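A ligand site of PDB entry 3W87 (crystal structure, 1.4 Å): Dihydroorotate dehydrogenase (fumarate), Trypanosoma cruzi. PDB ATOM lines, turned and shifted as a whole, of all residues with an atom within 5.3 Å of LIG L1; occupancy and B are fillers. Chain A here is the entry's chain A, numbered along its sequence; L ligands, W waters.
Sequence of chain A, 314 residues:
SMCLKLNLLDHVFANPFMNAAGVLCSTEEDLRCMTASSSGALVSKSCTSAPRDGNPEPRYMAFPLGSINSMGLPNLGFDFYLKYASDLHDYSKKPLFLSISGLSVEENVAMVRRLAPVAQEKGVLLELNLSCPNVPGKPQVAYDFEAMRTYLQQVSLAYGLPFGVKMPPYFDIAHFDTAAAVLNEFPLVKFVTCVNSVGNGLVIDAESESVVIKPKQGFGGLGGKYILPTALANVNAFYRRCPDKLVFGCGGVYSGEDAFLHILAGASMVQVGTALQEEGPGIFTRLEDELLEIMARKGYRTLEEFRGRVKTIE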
ATOM      1  N   LYS A  45      -1.146 -18.280  20.823  1.00  0.00           N
ATOM      2  CA  LYS A  45      -0.188 -18.595  21.921  1.00  0.00           C
ATOM      3  C   LYS A  45      -0.109 -20.100  22.051  1.00  0.00           C
ATOM      4  O   LYS A  45      -1.142 -20.819  21.994  1.00  0.00           O
ATOM      5  CB  LYS A  45      -0.819 -18.068  23.227  1.00  0.00           C
ATOM      6  CG  LYS A  45      -0.108 -18.516  24.512  1.00  0.00           C
ATOM      7  CD  LYS A  45       1.291 -17.994  24.615  1.00  0.00           C
ATOM      8  CE  LYS A  45       2.085 -18.667  25.757  1.00  0.00           C
ATOM      9  NZ  LYS A  45       3.526 -18.132  25.782  1.00  0.00           N
ATOM     10  N   SER A  46       1.059 -20.635  22.231  1.00  0.00           N
ATOM     11  CA  SER A  46       1.138 -22.119  22.465  1.00  0.00           C
ATOM     12  C   SER A  46       0.251 -22.504  23.683  1.00  0.00           C
ATOM     13  O   SER A  46       0.247 -21.860  24.739  1.00  0.00           O
ATOM     14  CB  SER A  46       2.551 -22.541  22.873  1.00  0.00           C
ATOM     15  OG  SER A  46       3.427 -22.370  21.724  1.00  0.00           O
ATOM     16  N   ARG A  52      -3.466 -22.211  31.951  1.00  0.00           N
ATOM     17  CA  ARG A  52      -2.383 -21.937  32.923  1.00  0.00           C
ATOM     18  C   ARG A  52      -2.205 -20.477  33.159  1.00  0.00           C
ATOM     19  O   ARG A  52      -2.278 -19.643  32.225  1.00  0.00           O
ATOM     20  CB  ARG A  52      -1.026 -22.403  32.348  1.00  0.00           C
ATOM     21  CG  ARG A  52      -0.860 -23.867  32.067  1.00  0.00           C
ATOM     22  CD  ARG A  52       0.436 -24.317  31.358  1.00  0.00           C
ATOM     23  NE  ARG A  52       1.628 -23.705  31.963  1.00  0.00           N
ATOM     24  CZ  ARG A  52       2.178 -24.215  33.036  1.00  0.00           C
ATOM     25  NH1 ARG A  52       1.771 -25.428  33.479  1.00  0.00           N
ATOM     26  NH2 ARG A  52       3.232 -23.618  33.590  1.00  0.00           N
ATOM     27  N   ASN A  55       4.132 -18.159  34.989  1.00  0.00           N
ATOM     28  CA  ASN A  55       5.029 -17.822  36.077  1.00  0.00           C
ATOM     29  C   ASN A  55       4.732 -16.506  36.712  1.00  0.00           C
ATOM     30  O   ASN A  55       4.058 -15.667  36.140  1.00  0.00           O
ATOM     31  CB  ASN A  55       6.462 -17.789  35.481  1.00  0.00           C
ATOM     32  CG  ASN A  55       6.980 -19.121  35.213  1.00  0.00           C
ATOM     33  OD1 ASN A  55       6.542 -20.151  35.786  1.00  0.00           O
ATOM     34  ND2 ASN A  55       7.991 -19.209  34.292  1.00  0.00           N
ATOM     35  N   ASN A  69      12.498 -13.518  28.384  1.00  0.00           N
ATOM     36  CA  ASN A  69      11.210 -13.982  28.989  1.00  0.00           C
ATOM     37  C   ASN A  69      11.305 -15.363  29.571  1.00  0.00           C
ATOM     38  O   ASN A  69      11.977 -16.242  29.099  1.00  0.00           O
ATOM     39  CB  ASN A  69      10.041 -13.948  27.995  1.00  0.00           C
ATOM     40  CG  ASN A  69       9.891 -15.254  27.163  1.00  0.00           C
ATOM     41  OD1 ASN A  69       9.289 -16.241  27.555  1.00  0.00           O
ATOM     42  ND2 ASN A  69      10.503 -15.278  25.970  1.00  0.00           N
ATOM     43  N   SER A  70      10.533 -15.540  30.656  1.00  0.00           N
ATOM     44  CA  SER A  70      10.190 -16.823  31.210  1.00  0.00           C
ATOM     45  C   SER A  70       8.741 -16.802  31.536  1.00  0.00           C
ATOM     46  O   SER A  70       8.370 -16.648  32.719  1.00  0.00           O
ATOM     47  CB  SER A  70      11.031 -17.145  32.450  1.00  0.00           C
ATOM     48  OG  SER A  70      10.754 -18.490  32.780  1.00  0.00           O
ATOM     49  N   MET A  71       7.903 -16.853  30.490  1.00  0.00           N
ATOM     50  CA  MET A  71       6.475 -16.672  30.702  1.00  0.00           C
ATOM     51  C   MET A  71       5.945 -17.834  31.473  1.00  0.00           C
ATOM     52  O   MET A  71       4.957 -17.597  32.268  1.00  0.00           O
ATOM     53  CB  MET A  71       5.739 -16.497  29.399  1.00  0.00           C
ATOM     54  CG  MET A  71       6.174 -15.350  28.473  1.00  0.00           C
ATOM     55  SD  MET A  71       6.179 -13.742  29.308  1.00  0.00           S
ATOM     56  CE  MET A  71       4.525 -13.382  29.302  1.00  0.00           C
ATOM     57  N   GLY A  72       6.417 -19.041  31.246  1.00  0.00           N
ATOM     58  CA  GLY A  72       5.784 -20.225  31.884  1.00  0.00           C
ATOM     59  C   GLY A  72       4.562 -20.705  31.185  1.00  0.00           C
ATOM     60  O   GLY A  72       3.722 -21.302  31.879  1.00  0.00           O
ATOM     61  N   LEU A  73       4.400 -20.489  29.884  1.00  0.00           N
ATOM     62  CA  LEU A  73       3.261 -21.034  29.134  1.00  0.00           C
ATOM     63  C   LEU A  73       1.918 -20.577  29.710  1.00  0.00           C
ATOM     64  O   LEU A  73       0.990 -21.444  29.790  1.00  0.00           O
ATOM     65  CB  LEU A  73       3.421 -22.570  29.037  1.00  0.00           C
ATOM     66  CG  LEU A  73       2.646 -23.366  28.074  1.00  0.00           C
ATOM     67  CD1 LEU A  73       2.601 -22.767  26.581  1.00  0.00           C
ATOM     68  CD2 LEU A  73       3.409 -24.724  27.954  1.00  0.00           C
ATOM     69  N   PRO A  74       1.776 -19.327  30.071  1.00  0.00           N
ATOM     70  CA  PRO A  74       0.373 -18.843  30.406  1.00  0.00           C
ATOM     71  C   PRO A  74      -0.487 -18.942  29.170  1.00  0.00           C
ATOM     72  O   PRO A  74      -0.110 -18.508  28.044  1.00  0.00           O
ATOM     73  CB  PRO A  74       0.551 -17.395  30.828  1.00  0.00           C
ATOM     74  CG  PRO A  74       1.881 -16.958  30.043  1.00  0.00           C
ATOM     75  CD  PRO A  74       2.742 -18.203  29.841  1.00  0.00           C
ATOM     76  N   SER A 101       1.666 -26.808  22.699  1.00  0.00           N
ATOM     77  CA  SER A 101       2.885 -27.140  23.519  1.00  0.00           C
ATOM     78  C   SER A 101       2.461 -27.927  24.746  1.00  0.00           C
ATOM     79  O   SER A 101       2.640 -27.449  25.845  1.00  0.00           O
ATOM     80  CB  SER A 101       3.694 -25.842  23.859  1.00  0.00           C
ATOM     81  OG  SER A 101       4.870 -26.211  24.401  1.00  0.00           O
ATOM     82  N   LEU A 103       2.548 -30.595  27.808  1.00  0.00           N
ATOM     83  CA  LEU A 103       3.676 -30.959  28.724  1.00  0.00           C
ATOM     84  C   LEU A 103       4.111 -32.443  28.543  1.00  0.00           C
ATOM     85  O   LEU A 103       5.108 -32.840  29.110  1.00  0.00           O
ATOM     86  CB  LEU A 103       3.273 -30.573  30.125  1.00  0.00           C
ATOM     87  CG  LEU A 103       2.763 -29.112  30.267  1.00  0.00           C
ATOM     88  CD1 LEU A 103       2.171 -28.750  31.634  1.00  0.00           C
ATOM     89  CD2 LEU A 103       3.839 -28.144  29.889  1.00  0.00           C
ATOM     90  N   ASN A 129       4.982 -26.888  18.940  1.00  0.00           N
ATOM     91  CA  ASN A 129       6.147 -26.269  19.622  1.00  0.00           C
ATOM     92  C   ASN A 129       6.992 -27.329  20.292  1.00  0.00           C
ATOM     93  O   ASN A 129       6.550 -27.889  21.260  1.00  0.00           O
ATOM     94  CB  ASN A 129       5.615 -25.241  20.595  1.00  0.00           C
ATOM     95  CG  ASN A 129       6.675 -24.496  21.342  1.00  0.00           C
ATOM     96  OD1 ASN A 129       7.846 -24.734  21.159  1.00  0.00           O
ATOM     97  ND2 ASN A 129       6.266 -23.590  22.193  1.00  0.00           N
ATOM     98  N   SER A 131       9.689 -27.035  21.879  1.00  0.00           N
ATOM     99  CA  SER A 131      10.238 -26.580  23.257  1.00  0.00           C
ATOM    100  C   SER A 131       9.412 -27.162  24.627  1.00  0.00           C
ATOM    101  O   SER A 131       8.240 -27.636  24.509  1.00  0.00           O
ATOM    102  CB  SER A 131      10.656 -25.038  23.104  1.00  0.00           C
ATOM    103  OG  SER A 131      11.788 -24.789  22.137  1.00  0.00           O
ATOM    104  N   CYS A 132       9.990 -27.174  25.853  1.00  0.00           N
ATOM    105  CA  CYS A 132       9.389 -27.881  27.067  1.00  0.00           C
ATOM    106  C   CYS A 132       9.822 -27.276  28.451  1.00  0.00           C
ATOM    107  O   CYS A 132      10.862 -26.596  28.519  1.00  0.00           O
ATOM    108  CB  CYS A 132       9.804 -29.378  27.063  1.00  0.00           C
ATOM    109  SG  CYS A 132       8.565 -30.637  27.557  1.00  0.00           S
ATOM    110  N   PRO A 133       9.048 -27.520  29.571  1.00  0.00           N
ATOM    111  CA  PRO A 133       9.650 -27.091  30.892  1.00  0.00           C
ATOM    112  C   PRO A 133      11.012 -27.798  31.160  1.00  0.00           C
ATOM    113  O   PRO A 133      11.281 -28.927  30.597  1.00  0.00           O
ATOM    114  CB  PRO A 133       8.631 -27.577  31.996  1.00  0.00           C
ATOM    115  CG  PRO A 133       7.658 -28.437  31.317  1.00  0.00           C
ATOM    116  CD  PRO A 133       7.735 -28.186  29.752  1.00  0.00           C
ATOM    117  N   ASN A 196      12.735 -20.470  17.845  1.00  0.00           N
ATOM    118  CA  ASN A 196      12.300 -20.018  19.201  1.00  0.00           C
ATOM    119  C   ASN A 196      13.424 -19.192  19.845  1.00  0.00           C
ATOM    120  O   ASN A 196      14.504 -18.973  19.298  1.00  0.00           O
ATOM    121  CB  ASN A 196      11.923 -21.296  20.023  1.00  0.00           C
ATOM    122  CG  ASN A 196      10.775 -21.034  20.968  1.00  0.00           C
ATOM    123  OD1 ASN A 196      10.778 -20.049  21.706  1.00  0.00           O
ATOM    124  ND2 ASN A 196       9.836 -21.915  21.005  1.00  0.00           N
ATOM    125  N   SER A 197      13.120 -18.715  21.045  1.00  0.00           N
ATOM    126  CA  SER A 197      14.106 -17.874  21.742  1.00  0.00           C
ATOM    127  C   SER A 197      15.376 -18.632  22.001  1.00  0.00           C
ATOM    128  O   SER A 197      15.455 -19.858  22.103  1.00  0.00           O
ATOM    129  CB  SER A 197      13.462 -17.298  23.028  1.00  0.00           C
ATOM    130  OG  SER A 197      12.875 -18.250  23.789  1.00  0.00           O
ATOM    131  N   PRO A 215      11.152 -15.410  37.527  1.00  0.00           N
ATOM    132  CA  PRO A 215      11.374 -16.844  37.446  1.00  0.00           C
ATOM    133  C   PRO A 215      12.777 -17.309  37.203  1.00  0.00           C
ATOM    134  O   PRO A 215      13.539 -16.533  36.600  1.00  0.00           O
ATOM    135  CB  PRO A 215      10.464 -17.350  36.267  1.00  0.00           C
ATOM    136  CG  PRO A 215       9.587 -16.199  36.014  1.00  0.00           C
ATOM    137  CD  PRO A 215      10.292 -14.923  36.434  1.00  0.00           C
ATOM    138  N   LYS A 216      13.105 -18.537  37.594  1.00  0.00           N
ATOM    139  CA  LYS A 216      14.361 -19.211  37.167  1.00  0.00           C
ATOM    140  C   LYS A 216      15.577 -18.363  37.517  1.00  0.00           C
ATOM    141  O   LYS A 216      16.554 -18.355  36.762  1.00  0.00           O
ATOM    142  CB  LYS A 216      14.353 -19.518  35.651  1.00  0.00           C
ATOM    143  CG  LYS A 216      13.305 -20.642  35.354  1.00  0.00           C
ATOM    144  CD  LYS A 216      13.191 -20.839  33.826  1.00  0.00           C
ATOM    145  CE  LYS A 216      14.591 -21.087  33.127  1.00  0.00           C
ATOM    146  NZ  LYS A 216      14.344 -21.516  31.697  1.00  0.00           N
ATOM    147  N   GLY A 221      14.506 -16.937  27.927  1.00  0.00           N
ATOM    148  CA  GLY A 221      14.817 -17.034  26.499  1.00  0.00           C
ATOM    149  C   GLY A 221      14.960 -15.640  25.948  1.00  0.00           C
ATOM    150  O   GLY A 221      14.221 -14.656  26.255  1.00  0.00           O
HETATM  151  O1  LIG L   1       5.591 -19.367  27.442  1.00  0.00           O
HETATM  152  C1  LIG L   1       6.864 -19.224  27.465  1.00  0.00           C
HETATM  153  O2  LIG L   1       7.616 -19.052  28.415  1.00  0.00           O
HETATM  154  C2  LIG L   1       7.544 -19.452  26.141  1.00  0.00           C
HETATM  155  N1  LIG L   1       8.560 -18.549  25.915  1.00  0.00           N
HETATM  156  C3  LIG L   1       9.311 -18.679  24.772  1.00  0.00           C
HETATM  157  O3  LIG L   1      10.242 -17.825  24.558  1.00  0.00           O
HETATM  158  N2  LIG L   1       9.133 -19.687  23.908  1.00  0.00           N
HETATM  159  C4  LIG L   1       8.127 -20.644  24.090  1.00  0.00           C
HETATM  160  O4  LIG L   1       8.053 -21.559  23.247  1.00  0.00           O
HETATM  161  C5  LIG L   1       7.296 -20.501  25.262  1.00  0.00           C
HETATM  162  C6  LIG L   1       6.204 -21.566  25.477  1.00  0.00           C
HETATM  163  C7  LIG L   1       6.850 -22.913  25.989  1.00  0.00           C
HETATM  164  C8  LIG L   1       7.770 -23.008  27.191  1.00  0.00           C
HETATM  165  C9  LIG L   1       7.440 -24.190  27.950  1.00  0.00           C
HETATM  166  C10 LIG L   1       7.632 -23.962  29.381  1.00  0.00           C
HETATM  167  C11 LIG L   1       6.762 -24.707  30.101  1.00  0.00           C
HETATM  168  C12 LIG L   1       8.551 -23.077  29.905  1.00  0.00           C
HETATM  169  C13 LIG L   1       8.662 -22.963  31.298  1.00  0.00           C
HETATM  170  C14 LIG L   1       7.761 -23.744  32.062  1.00  0.00           C
HETATM  171  C15 LIG L   1       6.855 -24.617  31.445  1.00  0.00           C
HETATM  172  C16 LIG L   1       5.995 -25.454  32.154  1.00  0.00           C
HETATM  173  C17 LIG L   1       6.119 -25.419  33.555  1.00  0.00           C
HETATM  174  C18 LIG L   1       7.009 -24.523  34.197  1.00  0.00           C
HETATM  175  C19 LIG L   1       7.844 -23.721  33.447  1.00  0.00           C
HETATM  176  C20 LIG L   1       8.725 -22.823  34.216  1.00  0.00           C
HETATM  177  O5  LIG L   1       9.263 -21.814  33.731  1.00  0.00           O
HETATM  178  O6  LIG L   1       8.808 -23.078  35.629  1.00  0.00           O
HETATM  179  C21 LIG L   1       9.691 -22.173  36.369  1.00  0.00           C
HETATM  180  N1  LG2 L   2       7.359 -19.288  21.068  1.00  0.00           N
HETATM  181  C1  LG2 L   2       6.433 -20.296  20.934  1.00  0.00           C
HETATM  182  O1  LG2 L   2       6.597 -21.096  20.033  1.00  0.00           O
HETATM  183  N2  LG2 L   2       5.304 -20.308  21.742  1.00  0.00           N
HETATM  184  C2  LG2 L   2       5.068 -19.368  22.639  1.00  0.00           C
HETATM  185  O2  LG2 L   2       3.972 -19.466  23.294  1.00  0.00           O
HETATM  186  C3  LG2 L   2       5.979 -18.350  22.878  1.00  0.00           C
HETATM  187  N3  LG2 L   2       5.717 -17.412  23.759  1.00  0.00           N
HETATM  188  C4  LG2 L   2       6.503 -16.277  23.750  1.00  0.00           C
HETATM  189  C5  LG2 L   2       6.242 -15.250  24.608  1.00  0.00           C
HETATM  190  C6  LG2 L   2       6.963 -14.064  24.610  1.00  0.00           C
HETATM  191  C7  LG2 L   2       6.680 -12.888  25.552  1.00  0.00           C
HETATM  192  C8  LG2 L   2       8.106 -13.981  23.796  1.00  0.00           C
HETATM  193  C9  LG2 L   2       8.976 -12.764  23.707  1.00  0.00           C
HETATM  194  C10 LG2 L   2       8.425 -15.019  22.929  1.00  0.00           C
HETATM  195  C11 LG2 L   2       7.641 -16.186  22.913  1.00  0.00           C
HETATM  196  N4  LG2 L   2       7.936 -17.261  22.084  1.00  0.00           N
HETATM  197  C12 LG2 L   2       7.089 -18.319  21.952  1.00  0.00           C
HETATM  198  C13 LG2 L   2       9.110 -17.179  21.151  1.00  0.00           C
HETATM  199  C14 LG2 L   2       8.808 -16.331  19.950  1.00  0.00           C
HETATM  200  O3  LG2 L   2       7.770 -16.969  19.173  1.00  0.00           O
HETATM  201  C15 LG2 L   2      10.000 -16.196  19.049  1.00  0.00           C
HETATM  202  O4  LG2 L   2      10.396 -17.514  18.607  1.00  0.00           O
HETATM  203  C16 LG2 L   2      11.185 -15.526  19.748  1.00  0.00           C
HETATM  204  O5  LG2 L   2      10.740 -14.450  20.587  1.00  0.00           O
HETATM  205  C17 LG2 L   2      12.211 -14.990  18.739  1.00  0.00           C
HETATM  206  O6  LG2 L   2      11.659 -14.030  17.851  1.00  0.00           O
HETATM  207  P1  LG2 L   2      11.944 -12.443  18.061  1.00  0.00           P
HETATM  208  O7  LG2 L   2      11.138 -11.802  17.000  1.00  0.00           O
HETATM  209  O8  LG2 L   2      13.428 -12.246  18.016  1.00  0.00           O
HETATM  210  O9  LG2 L   2      11.429 -12.098  19.457  1.00  0.00           O
HETATM  211  O   HOH W   1      11.615 -18.607  27.491  1.00  0.00           O
HETATM  212  O   HOH W   2      11.201 -24.680  33.694  1.00  0.00           O
HETATM  213  O   HOH W   3      10.102 -20.163  28.662  1.00  0.00           O
HETATM  214  O   HOH W   4      12.145 -22.984  38.472  1.00  0.00           O
HETATM  215  O   HOH W   5      11.234 -20.396  38.854  1.00  0.00           O
HETATM  216  O   HOH W   6       9.271 -19.980  31.290  1.00  0.00           O
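The side-chain amide nitrogen (ND2) of Asn 129 lies within hydrogen-bond range of an oxygen (O4) of LIG L1 (2.9 Å). The backbone NH of Gly 72 sits at hydrogen-bond distance from an oxygen (O2) of LIG L1. The side-chain hydroxyl (OG) of Ser 197 lies within hydrogen-bond range of an oxygen (O3) of LIG L1. N2 of LIG L1 is in hydrogen-bond range of OD1 of Asn 196. The side-chain amide nitrogen of Asn 129 sits at hydrogen-bond distance from an oxygen (O1) of LG2 L2 (3.3 Å). O2 of LG2 L2 sits at hydrogen-bond distance from NZ of Lys 45, 2.9 Å away. The side-chain amide nitrogen (ND2) of Asn 55 is in hydrogen-bond range of an oxygen (O5) of LIG L1, at 3.0 Å. The side-chain amide nitrogen of Asn 196 is in hydrogen-bond range of an oxygen (O1) of LG2 L2. OD1 of Asn 69 sits at hydrogen-bond distance from N1 of LIG L1, 2.9 Å away. The backbone NH (N) of Ser 46 sits at hydrogen-bond distance from an oxygen (O2) of LG2 L2 (3.3 Å). The backbone NH of Leu 73 sits at hydrogen-bond distance from an oxygen (O1) of LIG L1 (2.9 Å). O2 of LIG L1 sits at hydrogen-bond distance from N of Met 71, 3.0 Å away. A nitrogen (N2) of LG2 L2 is in hydrogen-bond range of the side-chain hydroxyl (OG) of Ser 46. NZ of Lys 45 is in salt-bridge range of O1 of LIG L1, at 2.9 Å.
N2 of LIG L1 sits close to N1 of LG2 L2, at 3.4 Å.
The backbone NH of Met 71 sits at hydrogen-bond distance from the side-chain amide oxygen of Asn 69 (3.3 Å). The side-chain amide nitrogen of Asn 55 lies within hydrogen-bond range of the backbone carbonyl oxygen of Ser 70 (3.0 Å). OD1 of Asn 129 is in hydrogen-bond range of ND2 of Asn 196 (3.5 Å). N of Gly 221 lies within hydrogen-bond range of O of Asn 69, 2.9 Å away. The backbone NH (N) of Gly 72 sits close to the side-chain amide nitrogen (ND2) of Asn 55, at 3.4 Å. The backbone carbonyl oxygen (O) of Met 71 sits at hydrogen-bond distance from the backbone NH (N) of Asn 55 (2.9 Å). The guanidinium group (NH2) of Arg 52 sits at hydrogen-bond distance from the backbone carbonyl oxygen (O) of Gly 72, 2.9 Å away. OD1 of Asn 196 lies within hydrogen-bond range of OG of Ser 197.
Arg 52 touches LIG L1. Ser 70 touches LIG L1. Pro 74 touches LIG L1 (CD to O1, 3.9 Å). Cys 132 touches LIG L1 (C to C9, 3.9 Å). Pro 133 touches LIG L1. Hydrophobic or aromatic side chains that line LIG L1: Met 71, Leu 73, Pro 74 and Pro 133. The nearest printed residue that does not touch LIG L1 is Lys 216 (4.05 Å).
Water W6 lies within hydrogen-bond range of OG of Ser 70 (2.6 Å), N of Gly 72 (3.0 Å), O5 of LIG L1 (3.1 Å) and ND2 of Asn 55 (3.4 Å). Water W1 lies within hydrogen-bond range of O of Asn 69 (2.9 Å), O3 of LIG L1 (3.3 Å) and N of Gly 221 (3.4 Å).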
